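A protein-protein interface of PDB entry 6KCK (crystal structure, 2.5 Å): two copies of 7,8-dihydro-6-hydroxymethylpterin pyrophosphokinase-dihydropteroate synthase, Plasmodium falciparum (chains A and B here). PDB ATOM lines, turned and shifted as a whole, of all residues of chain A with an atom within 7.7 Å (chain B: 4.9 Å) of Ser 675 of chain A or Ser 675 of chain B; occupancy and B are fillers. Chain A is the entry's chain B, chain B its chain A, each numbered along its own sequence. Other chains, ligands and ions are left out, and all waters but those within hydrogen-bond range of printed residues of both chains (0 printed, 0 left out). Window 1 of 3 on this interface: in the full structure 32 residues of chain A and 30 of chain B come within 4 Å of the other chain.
OG of Ser 675 of chain B lies within hydrogen-bond range of OG of Ser 675 of chain A.
O of Leu 671 of chain A sits at hydrogen-bond distance from OG of Ser 675 of chain A, 3.2 Å away. O of Leu 700 of chain B is in hydrogen-bond range of OH of Tyr 678 of chain B (3.5 Å). OG of Ser 675 of chain B sits at hydrogen-bond distance from O of Leu 671 of chain B (3.2 Å).
O of Cys 668 of chain A touches CG2 of Val 696 of chain B, at 3.4 Å. Leu 671 of chain B touches Leu 671 of chain A (CD1 to CD1, 3.7 Å). O of Val 696 of chain B touches CB of Ala 672 of chain A, 3.7 Å away. O of Ala 672 of chain A touches CD2 of Leu 700 of chain B (3.5 Å). Tyr 679 of chain B touches Tyr 676 of chain A (OH to CD1, 3.4 Å). Tyr 676 of chain B touches Tyr 679 of chain A (CD1 to OH, 3.3 Å). O of Val 696 of chain A touches CB of Ala 672 of chain B, at 3.5 Å. O of Ala 672 of chain B touches CD2 of Leu 700 of chain A (3.6 Å).
Ser 675 of chain A touches one residue of chain B. Of chain A, only Ser 675 (2.8 Å) comes within 4 Å of Ser 675 of chain B. No residue of chain A comes within 4 Å of Ala 674 of chain B. Printed residues of chain B within 4 Å of Leu 700 of chain A: Ala 672 (3.6 Å). Printed residues of chain B within 4 Å of Tyr 676 of chain A: Tyr 679 (3.4 Å). Of the printed residues of chain B, Ala 672 of chain A touches Val 696 (3.7 Å) and Leu 700 (3.5 Å). Ile 685 of chain A touches none of the printed residues of chain B. The nearest residue of chain A that does not touch Ser 675 of chain B is Ala 672 of chain A (4.6 Å). The nearest printed residue of chain B that does not touch Val 696 of chain A is Leu 671 of chain B (4.7 Å).
Of the 11 printed residues of chain B, 7 touch a printed residue of chain A. Printed residues of chain B that touch a printed residue of chain A: Leu 671, Ala 672, Ser 675, Tyr 676, Tyr 679, Val 696 and Leu 700. Hydrophobic or aromatic side chains of chain B that line the printed part of chain A: Leu 671, Ala 672, Tyr 676, Tyr 679, Val 696 and Leu 700. Printed residues of chain A that touch a printed residue of chain B: Cys 668, Leu 671, Ala 672, Ser 675, Tyr 676, Tyr 679, Val 696 and Leu 700. Hydrophobic or aromatic side chains of chain A within 4 Å of the printed part of chain B: Leu 671, Ala 672, Tyr 676, Tyr 679, Val 696 and Leu 700.
Leu 671 of chain A touches its own counterpart, Leu 671 of chain B. Ala 672 of chain A touches Val 696 of chain B, and with the chains exchanged Val 696 of chain A touches Ala 672 of chain B. Ser 675 of chain A touches its own counterpart, Ser 675 of chain B. Tyr 676 of chain A touches Tyr 679 of chain B, and with the chains exchanged Tyr 679 of chain A touches Tyr 676 of chain B. Of the 9 pairs that touch across the chains among the printed residues, 8 have their exchanged pair printed and touching as well.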
ATOM      1  N   THR A 389     -25.880  11.243 -24.439  1.00  0.00           N
ATOM      2  CA  THR A 389     -26.111  10.972 -23.043  1.00  0.00           C
ATOM      3  C   THR A 389     -25.853  12.240 -22.253  1.00  0.00           C
ATOM      4  O   THR A 389     -24.716  12.656 -22.112  1.00  0.00           O
ATOM      5  CB  THR A 389     -25.208   9.844 -22.579  1.00  0.00           C
ATOM      6  OG1 THR A 389     -25.649   8.645 -23.210  1.00  0.00           O
ATOM      7  CG2 THR A 389     -25.289   9.681 -21.074  1.00  0.00           C
ATOM      8  N   TYR A 606     -27.954   5.859 -11.048  1.00  0.00           N
ATOM      9  CA  TYR A 606     -27.225   4.812 -10.350  1.00  0.00           C
ATOM     10  C   TYR A 606     -26.259   5.427  -9.329  1.00  0.00           C
ATOM     11  O   TYR A 606     -25.742   4.765  -8.435  1.00  0.00           O
ATOM     12  CB  TYR A 606     -26.407   4.038 -11.379  1.00  0.00           C
ATOM     13  CG  TYR A 606     -25.521   4.950 -12.231  1.00  0.00           C
ATOM     14  CD1 TYR A 606     -24.310   5.489 -11.722  1.00  0.00           C
ATOM     15  CD2 TYR A 606     -25.895   5.280 -13.538  1.00  0.00           C
ATOM     16  CE1 TYR A 606     -23.507   6.325 -12.500  1.00  0.00           C
ATOM     17  CE2 TYR A 606     -25.096   6.092 -14.317  1.00  0.00           C
ATOM     18  CZ  TYR A 606     -23.906   6.602 -13.810  1.00  0.00           C
ATOM     19  OH  TYR A 606     -23.150   7.429 -14.628  1.00  0.00           O
ATOM     20  N   CYS A 668     -15.902   5.422  -8.934  1.00  0.00           N
ATOM     21  CA  CYS A 668     -15.350   4.698 -10.061  1.00  0.00           C
ATOM     22  C   CYS A 668     -16.305   3.634 -10.662  1.00  0.00           C
ATOM     23  O   CYS A 668     -16.465   3.543 -11.899  1.00  0.00           O
ATOM     24  CB  CYS A 668     -13.964   4.140  -9.700  1.00  0.00           C
ATOM     25  SG  CYS A 668     -12.778   5.490  -9.387  1.00  0.00           S
ATOM     26  N   GLY A 669     -16.959   2.862  -9.802  1.00  0.00           N
ATOM     27  CA  GLY A 669     -18.011   1.934 -10.234  1.00  0.00           C
ATOM     28  C   GLY A 669     -19.075   2.633 -11.073  1.00  0.00           C
ATOM     29  O   GLY A 669     -19.494   2.117 -12.118  1.00  0.00           O
ATOM     30  N   GLY A 670     -19.480   3.826 -10.644  1.00  0.00           N
ATOM     31  CA  GLY A 670     -20.423   4.644 -11.389  1.00  0.00           C
ATOM     32  C   GLY A 670     -19.993   5.022 -12.794  1.00  0.00           C
ATOM     33  O   GLY A 670     -20.798   4.975 -13.751  1.00  0.00           O
ATOM     34  N   LEU A 671     -18.720   5.412 -12.915  1.00  0.00           N
ATOM     35  CA  LEU A 671     -18.115   5.821 -14.185  1.00  0.00           C
ATOM     36  C   LEU A 671     -18.185   4.674 -15.179  1.00  0.00           C
ATOM     37  O   LEU A 671     -18.385   4.885 -16.386  1.00  0.00           O
ATOM     38  CB  LEU A 671     -16.659   6.269 -13.953  1.00  0.00           C
ATOM     39  CG  LEU A 671     -16.502   7.571 -13.149  1.00  0.00           C
ATOM     40  CD1 LEU A 671     -15.021   7.872 -12.952  1.00  0.00           C
ATOM     41  CD2 LEU A 671     -17.190   8.725 -13.859  1.00  0.00           C
ATOM     42  N   ALA A 672     -18.086   3.454 -14.651  1.00  0.00           N
ATOM     43  CA  ALA A 672     -18.376   2.266 -15.451  1.00  0.00           C
ATOM     44  C   ALA A 672     -19.827   2.250 -15.947  1.00  0.00           C
ATOM     45  O   ALA A 672     -20.091   1.888 -17.104  1.00  0.00           O
ATOM     46  CB  ALA A 672     -18.060   0.993 -14.660  1.00  0.00           C
ATOM     47  N   ILE A 673     -20.781   2.635 -15.102  1.00  0.00           N
ATOM     48  CA  ILE A 673     -22.150   2.614 -15.558  1.00  0.00           C
ATOM     49  C   ILE A 673     -22.379   3.760 -16.508  1.00  0.00           C
ATOM     50  O   ILE A 673     -23.170   3.637 -17.449  1.00  0.00           O
ATOM     51  CB  ILE A 673     -23.170   2.592 -14.405  1.00  0.00           C
ATOM     52  CG1 ILE A 673     -22.908   1.332 -13.572  1.00  0.00           C
ATOM     53  CG2 ILE A 673     -24.580   2.535 -14.953  1.00  0.00           C
ATOM     54  CD1 ILE A 673     -23.464   1.346 -12.175  1.00  0.00           C
ATOM     55  N   ALA A 674     -21.676   4.865 -16.288  1.00  0.00           N
ATOM     56  CA  ALA A 674     -21.663   5.943 -17.266  1.00  0.00           C
ATOM     57  C   ALA A 674     -21.230   5.433 -18.657  1.00  0.00           C
ATOM     58  O   ALA A 674     -21.847   5.781 -19.672  1.00  0.00           O
ATOM     59  CB  ALA A 674     -20.759   7.086 -16.802  1.00  0.00           C
ATOM     60  N   SER A 675     -20.180   4.615 -18.706  1.00  0.00           N
ATOM     61  CA  SER A 675     -19.688   4.095 -19.989  1.00  0.00           C
ATOM     62  C   SER A 675     -20.745   3.185 -20.608  1.00  0.00           C
ATOM     63  O   SER A 675     -21.081   3.301 -21.804  1.00  0.00           O
ATOM     64  CB  SER A 675     -18.399   3.276 -19.815  1.00  0.00           C
ATOM     65  OG  SER A 675     -17.369   4.097 -19.315  1.00  0.00           O
ATOM     66  N   TYR A 676     -21.242   2.262 -19.787  1.00  0.00           N
ATOM     67  CA  TYR A 676     -22.231   1.316 -20.246  1.00  0.00           C
ATOM     68  C   TYR A 676     -23.404   2.113 -20.763  1.00  0.00           C
ATOM     69  O   TYR A 676     -23.888   1.834 -21.850  1.00  0.00           O
ATOM     70  CB  TYR A 676     -22.651   0.408 -19.096  1.00  0.00           C
ATOM     71  CG  TYR A 676     -23.746  -0.562 -19.437  1.00  0.00           C
ATOM     72  CD1 TYR A 676     -23.462  -1.725 -20.147  1.00  0.00           C
ATOM     73  CD2 TYR A 676     -25.088  -0.323 -19.023  1.00  0.00           C
ATOM     74  CE1 TYR A 676     -24.454  -2.627 -20.441  1.00  0.00           C
ATOM     75  CE2 TYR A 676     -26.103  -1.224 -19.322  1.00  0.00           C
ATOM     76  CZ  TYR A 676     -25.779  -2.375 -20.016  1.00  0.00           C
ATOM     77  OH  TYR A 676     -26.750  -3.281 -20.331  1.00  0.00           O
ATOM     78  N   SER A 677     -23.822   3.132 -20.006  1.00  0.00           N
ATOM     79  CA  SER A 677     -24.948   3.987 -20.366  1.00  0.00           C
ATOM     80  C   SER A 677     -24.664   4.683 -21.681  1.00  0.00           C
ATOM     81  O   SER A 677     -25.545   4.772 -22.548  1.00  0.00           O
ATOM     82  CB  SER A 677     -25.192   5.048 -19.287  1.00  0.00           C
ATOM     83  OG  SER A 677     -25.751   4.484 -18.115  1.00  0.00           O
ATOM     84  N   TYR A 678     -23.427   5.164 -21.838  1.00  0.00           N
ATOM     85  CA  TYR A 678     -23.047   5.802 -23.051  1.00  0.00           C
ATOM     86  C   TYR A 678     -23.262   4.868 -24.235  1.00  0.00           C
ATOM     87  O   TYR A 678     -23.807   5.290 -25.274  1.00  0.00           O
ATOM     88  CB  TYR A 678     -21.587   6.280 -22.998  1.00  0.00           C
ATOM     89  CG  TYR A 678     -21.104   6.715 -24.361  1.00  0.00           C
ATOM     90  CD1 TYR A 678     -20.546   5.783 -25.241  1.00  0.00           C
ATOM     91  CD2 TYR A 678     -21.239   8.046 -24.793  1.00  0.00           C
ATOM     92  CE1 TYR A 678     -20.125   6.152 -26.504  1.00  0.00           C
ATOM     93  CE2 TYR A 678     -20.816   8.433 -26.059  1.00  0.00           C
ATOM     94  CZ  TYR A 678     -20.273   7.466 -26.911  1.00  0.00           C
ATOM     95  OH  TYR A 678     -19.827   7.788 -28.171  1.00  0.00           O
ATOM     96  N   TYR A 679     -22.838   3.611 -24.099  1.00  0.00           N
ATOM     97  CA  TYR A 679     -22.934   2.677 -25.223  1.00  0.00           C
ATOM     98  C   TYR A 679     -24.346   2.189 -25.401  1.00  0.00           C
ATOM     99  O   TYR A 679     -24.736   1.842 -26.507  1.00  0.00           O
ATOM    100  CB  TYR A 679     -21.981   1.494 -25.075  1.00  0.00           C
ATOM    101  CG  TYR A 679     -20.516   1.876 -25.280  1.00  0.00           C
ATOM    102  CD1 TYR A 679     -20.046   2.315 -26.543  1.00  0.00           C
ATOM    103  CD2 TYR A 679     -19.613   1.798 -24.241  1.00  0.00           C
ATOM    104  CE1 TYR A 679     -18.723   2.656 -26.735  1.00  0.00           C
ATOM    105  CE2 TYR A 679     -18.278   2.148 -24.430  1.00  0.00           C
ATOM    106  CZ  TYR A 679     -17.845   2.560 -25.671  1.00  0.00           C
ATOM    107  OH  TYR A 679     -16.518   2.889 -25.842  1.00  0.00           O
ATOM    108  N   LYS A 680     -25.129   2.174 -24.318  1.00  0.00           N
ATOM    109  CA  LYS A 680     -26.522   1.787 -24.469  1.00  0.00           C
ATOM    110  C   LYS A 680     -27.372   2.967 -24.912  1.00  0.00           C
ATOM    111  O   LYS A 680     -28.565   2.831 -25.090  1.00  0.00           O
ATOM    112  CB  LYS A 680     -27.068   1.132 -23.209  1.00  0.00           C
ATOM    113  CG  LYS A 680     -26.528  -0.262 -23.002  1.00  0.00           C
ATOM    114  CD  LYS A 680     -26.880  -1.185 -24.156  1.00  0.00           C
ATOM    115  CE  LYS A 680     -26.402  -2.586 -23.831  1.00  0.00           C
ATOM    116  NZ  LYS A 680     -27.175  -3.628 -24.576  1.00  0.00           N
ATOM    117  N   LYS A 681     -26.734   4.125 -25.066  1.00  0.00           N
ATOM    118  CA  LYS A 681     -27.390   5.334 -25.539  1.00  0.00           C
ATOM    119  C   LYS A 681     -28.506   5.829 -24.646  1.00  0.00           C
ATOM    120  O   LYS A 681     -29.488   6.368 -25.137  1.00  0.00           O
ATOM    121  CB  LYS A 681     -27.907   5.142 -26.958  1.00  0.00           C
ATOM    122  CG  LYS A 681     -26.779   4.833 -27.922  1.00  0.00           C
ATOM    123  CD  LYS A 681     -27.299   4.476 -29.291  1.00  0.00           C
ATOM    124  CE  LYS A 681     -26.149   4.363 -30.274  1.00  0.00           C
ATOM    125  NZ  LYS A 681     -26.774   4.381 -31.628  1.00  0.00           N
ATOM    126  N   ILE A 685     -28.412  10.678 -17.463  1.00  0.00           N
ATOM    127  CA  ILE A 685     -27.897  10.023 -16.297  1.00  0.00           C
ATOM    128  C   ILE A 685     -27.724  11.082 -15.207  1.00  0.00           C
ATOM    129  O   ILE A 685     -27.138  12.168 -15.431  1.00  0.00           O
ATOM    130  CB  ILE A 685     -26.578   9.260 -16.580  1.00  0.00           C
ATOM    131  CG1 ILE A 685     -25.534  10.176 -17.238  1.00  0.00           C
ATOM    132  CG2 ILE A 685     -26.842   8.032 -17.459  1.00  0.00           C
ATOM    133  CD1 ILE A 685     -24.158   9.555 -17.324  1.00  0.00           C
ATOM    134  N   THR A 693     -17.744  12.385 -14.707  1.00  0.00           N
ATOM    135  CA  THR A 693     -18.641  11.763 -15.679  1.00  0.00           C
ATOM    136  C   THR A 693     -18.432  12.388 -17.073  1.00  0.00           C
ATOM    137  O   THR A 693     -18.340  11.677 -18.092  1.00  0.00           O
ATOM    138  CB  THR A 693     -20.145  11.841 -15.211  1.00  0.00           C
ATOM    139  OG1 THR A 693     -20.287  11.186 -13.939  1.00  0.00           O
ATOM    140  CG2 THR A 693     -21.056  11.186 -16.187  1.00  0.00           C
ATOM    141  N   VAL A 696     -15.285  11.128 -18.629  1.00  0.00           N
ATOM    142  CA  VAL A 696     -15.540   9.827 -19.202  1.00  0.00           C
ATOM    143  C   VAL A 696     -16.279   9.950 -20.549  1.00  0.00           C
ATOM    144  O   VAL A 696     -15.849   9.374 -21.541  1.00  0.00           O
ATOM    145  CB  VAL A 696     -16.245   8.875 -18.195  1.00  0.00           C
ATOM    146  CG1 VAL A 696     -16.768   7.623 -18.895  1.00  0.00           C
ATOM    147  CG2 VAL A 696     -15.275   8.502 -17.079  1.00  0.00           C
ATOM    148  N   LEU A 697     -17.354  10.717 -20.597  1.00  0.00           N
ATOM    149  CA  LEU A 697     -18.192  10.770 -21.796  1.00  0.00           C
ATOM    150  C   LEU A 697     -17.463  11.431 -22.934  1.00  0.00           C
ATOM    151  O   LEU A 697     -17.636  11.023 -24.093  1.00  0.00           O
ATOM    152  CB  LEU A 697     -19.525  11.475 -21.522  1.00  0.00           C
ATOM    153  CG  LEU A 697     -20.499  10.759 -20.559  1.00  0.00           C
ATOM    154  CD1 LEU A 697     -21.829  11.468 -20.416  1.00  0.00           C
ATOM    155  CD2 LEU A 697     -20.781   9.331 -20.948  1.00  0.00           C
ATOM    156  N   LEU A 700     -15.044   8.791 -24.457  1.00  0.00           N
ATOM    157  CA  LEU A 700     -15.802   7.795 -25.230  1.00  0.00           C
ATOM    158  C   LEU A 700     -16.337   8.379 -26.538  1.00  0.00           C
ATOM    159  O   LEU A 700     -16.324   7.717 -27.568  1.00  0.00           O
ATOM    160  CB  LEU A 700     -16.941   7.206 -24.402  1.00  0.00           C
ATOM    161  CG  LEU A 700     -16.490   6.382 -23.193  1.00  0.00           C
ATOM    162  CD1 LEU A 700     -17.669   5.885 -22.381  1.00  0.00           C
ATOM    163  CD2 LEU A 700     -15.684   5.186 -23.633  1.00  0.00           C
ATOM    164  N   LEU B 671     -10.306   5.920 -17.264  1.00  0.00           N
ATOM    165  CA  LEU B 671     -11.345   4.941 -16.936  1.00  0.00           C
ATOM    166  C   LEU B 671     -12.265   4.716 -18.129  1.00  0.00           C
ATOM    167  O   LEU B 671     -12.663   3.581 -18.363  1.00  0.00           O
ATOM    168  CB  LEU B 671     -12.101   5.313 -15.670  1.00  0.00           C
ATOM    169  CG  LEU B 671     -11.088   5.439 -14.507  1.00  0.00           C
ATOM    170  CD1 LEU B 671     -11.780   6.090 -13.313  1.00  0.00           C
ATOM    171  CD2 LEU B 671     -10.448   4.098 -14.151  1.00  0.00           C
ATOM    172  N   ALA B 672     -12.546   5.768 -18.914  1.00  0.00           N
ATOM    173  CA  ALA B 672     -13.220   5.571 -20.203  1.00  0.00           C
ATOM    174  C   ALA B 672     -12.483   4.596 -21.114  1.00  0.00           C
ATOM    175  O   ALA B 672     -13.103   3.664 -21.643  1.00  0.00           O
ATOM    176  CB  ALA B 672     -13.454   6.878 -20.913  1.00  0.00           C
ATOM    177  N   ILE B 673     -11.169   4.768 -21.276  1.00  0.00           N
ATOM    178  CA  ILE B 673     -10.396   3.858 -22.106  1.00  0.00           C
ATOM    179  C   ILE B 673     -10.325   2.433 -21.502  1.00  0.00           C
ATOM    180  O   ILE B 673     -10.296   1.445 -22.264  1.00  0.00           O
ATOM    181  CB  ILE B 673      -8.989   4.407 -22.456  1.00  0.00           C
ATOM    182  CG1 ILE B 673      -9.077   5.867 -22.913  1.00  0.00           C
ATOM    183  CG2 ILE B 673      -8.326   3.540 -23.524  1.00  0.00           C
ATOM    184  CD1 ILE B 673      -7.737   6.437 -23.348  1.00  0.00           C
ATOM    185  N   ALA B 674     -10.322   2.315 -20.164  1.00  0.00           N
ATOM    186  CA  ALA B 674     -10.544   0.989 -19.525  1.00  0.00           C
ATOM    187  C   ALA B 674     -11.879   0.349 -19.934  1.00  0.00           C
ATOM    188  O   ALA B 674     -11.916  -0.848 -20.214  1.00  0.00           O
ATOM    189  CB  ALA B 674     -10.455   1.058 -18.004  1.00  0.00           C
ATOM    190  N   SER B 675     -12.963   1.137 -19.965  1.00  0.00           N
ATOM    191  CA  SER B 675     -14.256   0.622 -20.424  1.00  0.00           C
ATOM    192  C   SER B 675     -14.173   0.159 -21.881  1.00  0.00           C
ATOM    193  O   SER B 675     -14.594  -0.948 -22.233  1.00  0.00           O
ATOM    194  CB  SER B 675     -15.336   1.680 -20.333  1.00  0.00           C
ATOM    195  OG  SER B 675     -15.443   2.107 -19.009  1.00  0.00           O
ATOM    196  N   TYR B 676     -13.632   1.032 -22.718  1.00  0.00           N
ATOM    197  CA  TYR B 676     -13.484   0.719 -24.118  1.00  0.00           C
ATOM    198  C   TYR B 676     -12.666  -0.549 -24.265  1.00  0.00           C
ATOM    199  O   TYR B 676     -13.055  -1.453 -25.018  1.00  0.00           O
ATOM    200  CB  TYR B 676     -12.789   1.873 -24.810  1.00  0.00           C
ATOM    201  CG  TYR B 676     -12.630   1.688 -26.286  1.00  0.00           C
ATOM    202  CD1 TYR B 676     -13.743   1.714 -27.154  1.00  0.00           C
ATOM    203  CD2 TYR B 676     -11.368   1.549 -26.834  1.00  0.00           C
ATOM    204  CE1 TYR B 676     -13.572   1.566 -28.522  1.00  0.00           C
ATOM    205  CE2 TYR B 676     -11.187   1.405 -28.193  1.00  0.00           C
ATOM    206  CZ  TYR B 676     -12.274   1.422 -29.028  1.00  0.00           C
ATOM    207  OH  TYR B 676     -12.035   1.278 -30.374  1.00  0.00           O
ATOM    208  N   SER B 677     -11.563  -0.618 -23.514  1.00  0.00           N
ATOM    209  CA  SER B 677     -10.625  -1.731 -23.592  1.00  0.00           C
ATOM    210  C   SER B 677     -11.299  -3.017 -23.212  1.00  0.00           C
ATOM    211  O   SER B 677     -11.154  -4.041 -23.900  1.00  0.00           O
ATOM    212  CB  SER B 677      -9.419  -1.498 -22.681  1.00  0.00           C
ATOM    213  OG  SER B 677      -8.640  -0.437 -23.214  1.00  0.00           O
ATOM    214  N   TYR B 678     -12.049  -2.953 -22.118  1.00  0.00           N
ATOM    215  CA  TYR B 678     -12.832  -4.070 -21.652  1.00  0.00           C
ATOM    216  C   TYR B 678     -13.743  -4.620 -22.749  1.00  0.00           C
ATOM    217  O   TYR B 678     -13.782  -5.833 -22.981  1.00  0.00           O
ATOM    218  CB  TYR B 678     -13.681  -3.663 -20.432  1.00  0.00           C
ATOM    219  CG  TYR B 678     -14.678  -4.730 -20.098  1.00  0.00           C
ATOM    220  CD1 TYR B 678     -15.974  -4.701 -20.621  1.00  0.00           C
ATOM    221  CD2 TYR B 678     -14.300  -5.801 -19.293  1.00  0.00           C
ATOM    222  CE1 TYR B 678     -16.865  -5.719 -20.321  1.00  0.00           C
ATOM    223  CE2 TYR B 678     -15.167  -6.816 -18.985  1.00  0.00           C
ATOM    224  CZ  TYR B 678     -16.431  -6.785 -19.500  1.00  0.00           C
ATOM    225  OH  TYR B 678     -17.251  -7.826 -19.169  1.00  0.00           O
ATOM    226  N   TYR B 679     -14.487  -3.745 -23.412  1.00  0.00           N
ATOM    227  CA  TYR B 679     -15.346  -4.218 -24.473  1.00  0.00           C
ATOM    228  C   TYR B 679     -14.585  -4.678 -25.682  1.00  0.00           C
ATOM    229  O   TYR B 679     -15.094  -5.461 -26.444  1.00  0.00           O
ATOM    230  CB  TYR B 679     -16.348  -3.151 -24.887  1.00  0.00           C
ATOM    231  CG  TYR B 679     -17.385  -2.949 -23.815  1.00  0.00           C
ATOM    232  CD1 TYR B 679     -18.245  -3.986 -23.480  1.00  0.00           C
ATOM    233  CD2 TYR B 679     -17.494  -1.732 -23.130  1.00  0.00           C
ATOM    234  CE1 TYR B 679     -19.188  -3.830 -22.491  1.00  0.00           C
ATOM    235  CE2 TYR B 679     -18.435  -1.575 -22.138  1.00  0.00           C
ATOM    236  CZ  TYR B 679     -19.276  -2.643 -21.827  1.00  0.00           C
ATOM    237  OH  TYR B 679     -20.235  -2.543 -20.820  1.00  0.00           O
ATOM    238  N   VAL B 696     -13.852  -0.314 -12.135  1.00  0.00           N
ATOM    239  CA  VAL B 696     -14.534  -0.203 -13.403  1.00  0.00           C
ATOM    240  C   VAL B 696     -14.695  -1.586 -13.971  1.00  0.00           C
ATOM    241  O   VAL B 696     -15.792  -1.964 -14.340  1.00  0.00           O
ATOM    242  CB  VAL B 696     -13.839   0.770 -14.388  1.00  0.00           C
ATOM    243  CG1 VAL B 696     -14.360   0.540 -15.798  1.00  0.00           C
ATOM    244  CG2 VAL B 696     -14.086   2.219 -13.970  1.00  0.00           C
ATOM    245  N   LEU B 700     -18.273  -3.694 -14.891  1.00  0.00           N
ATOM    246  CA  LEU B 700     -18.660  -4.023 -16.248  1.00  0.00           C
ATOM    247  C   LEU B 700     -18.762  -5.532 -16.430  1.00  0.00           C
ATOM    248  O   LEU B 700     -19.553  -6.024 -17.258  1.00  0.00           O
ATOM    249  CB  LEU B 700     -17.640  -3.461 -17.240  1.00  0.00           C
ATOM    250  CG  LEU B 700     -17.468  -1.939 -17.360  1.00  0.00           C
ATOM    251  CD1 LEU B 700     -16.393  -1.630 -18.380  1.00  0.00           C
ATOM    252  CD2 LEU B 700     -18.758  -1.247 -17.757  1.00  0.00           C
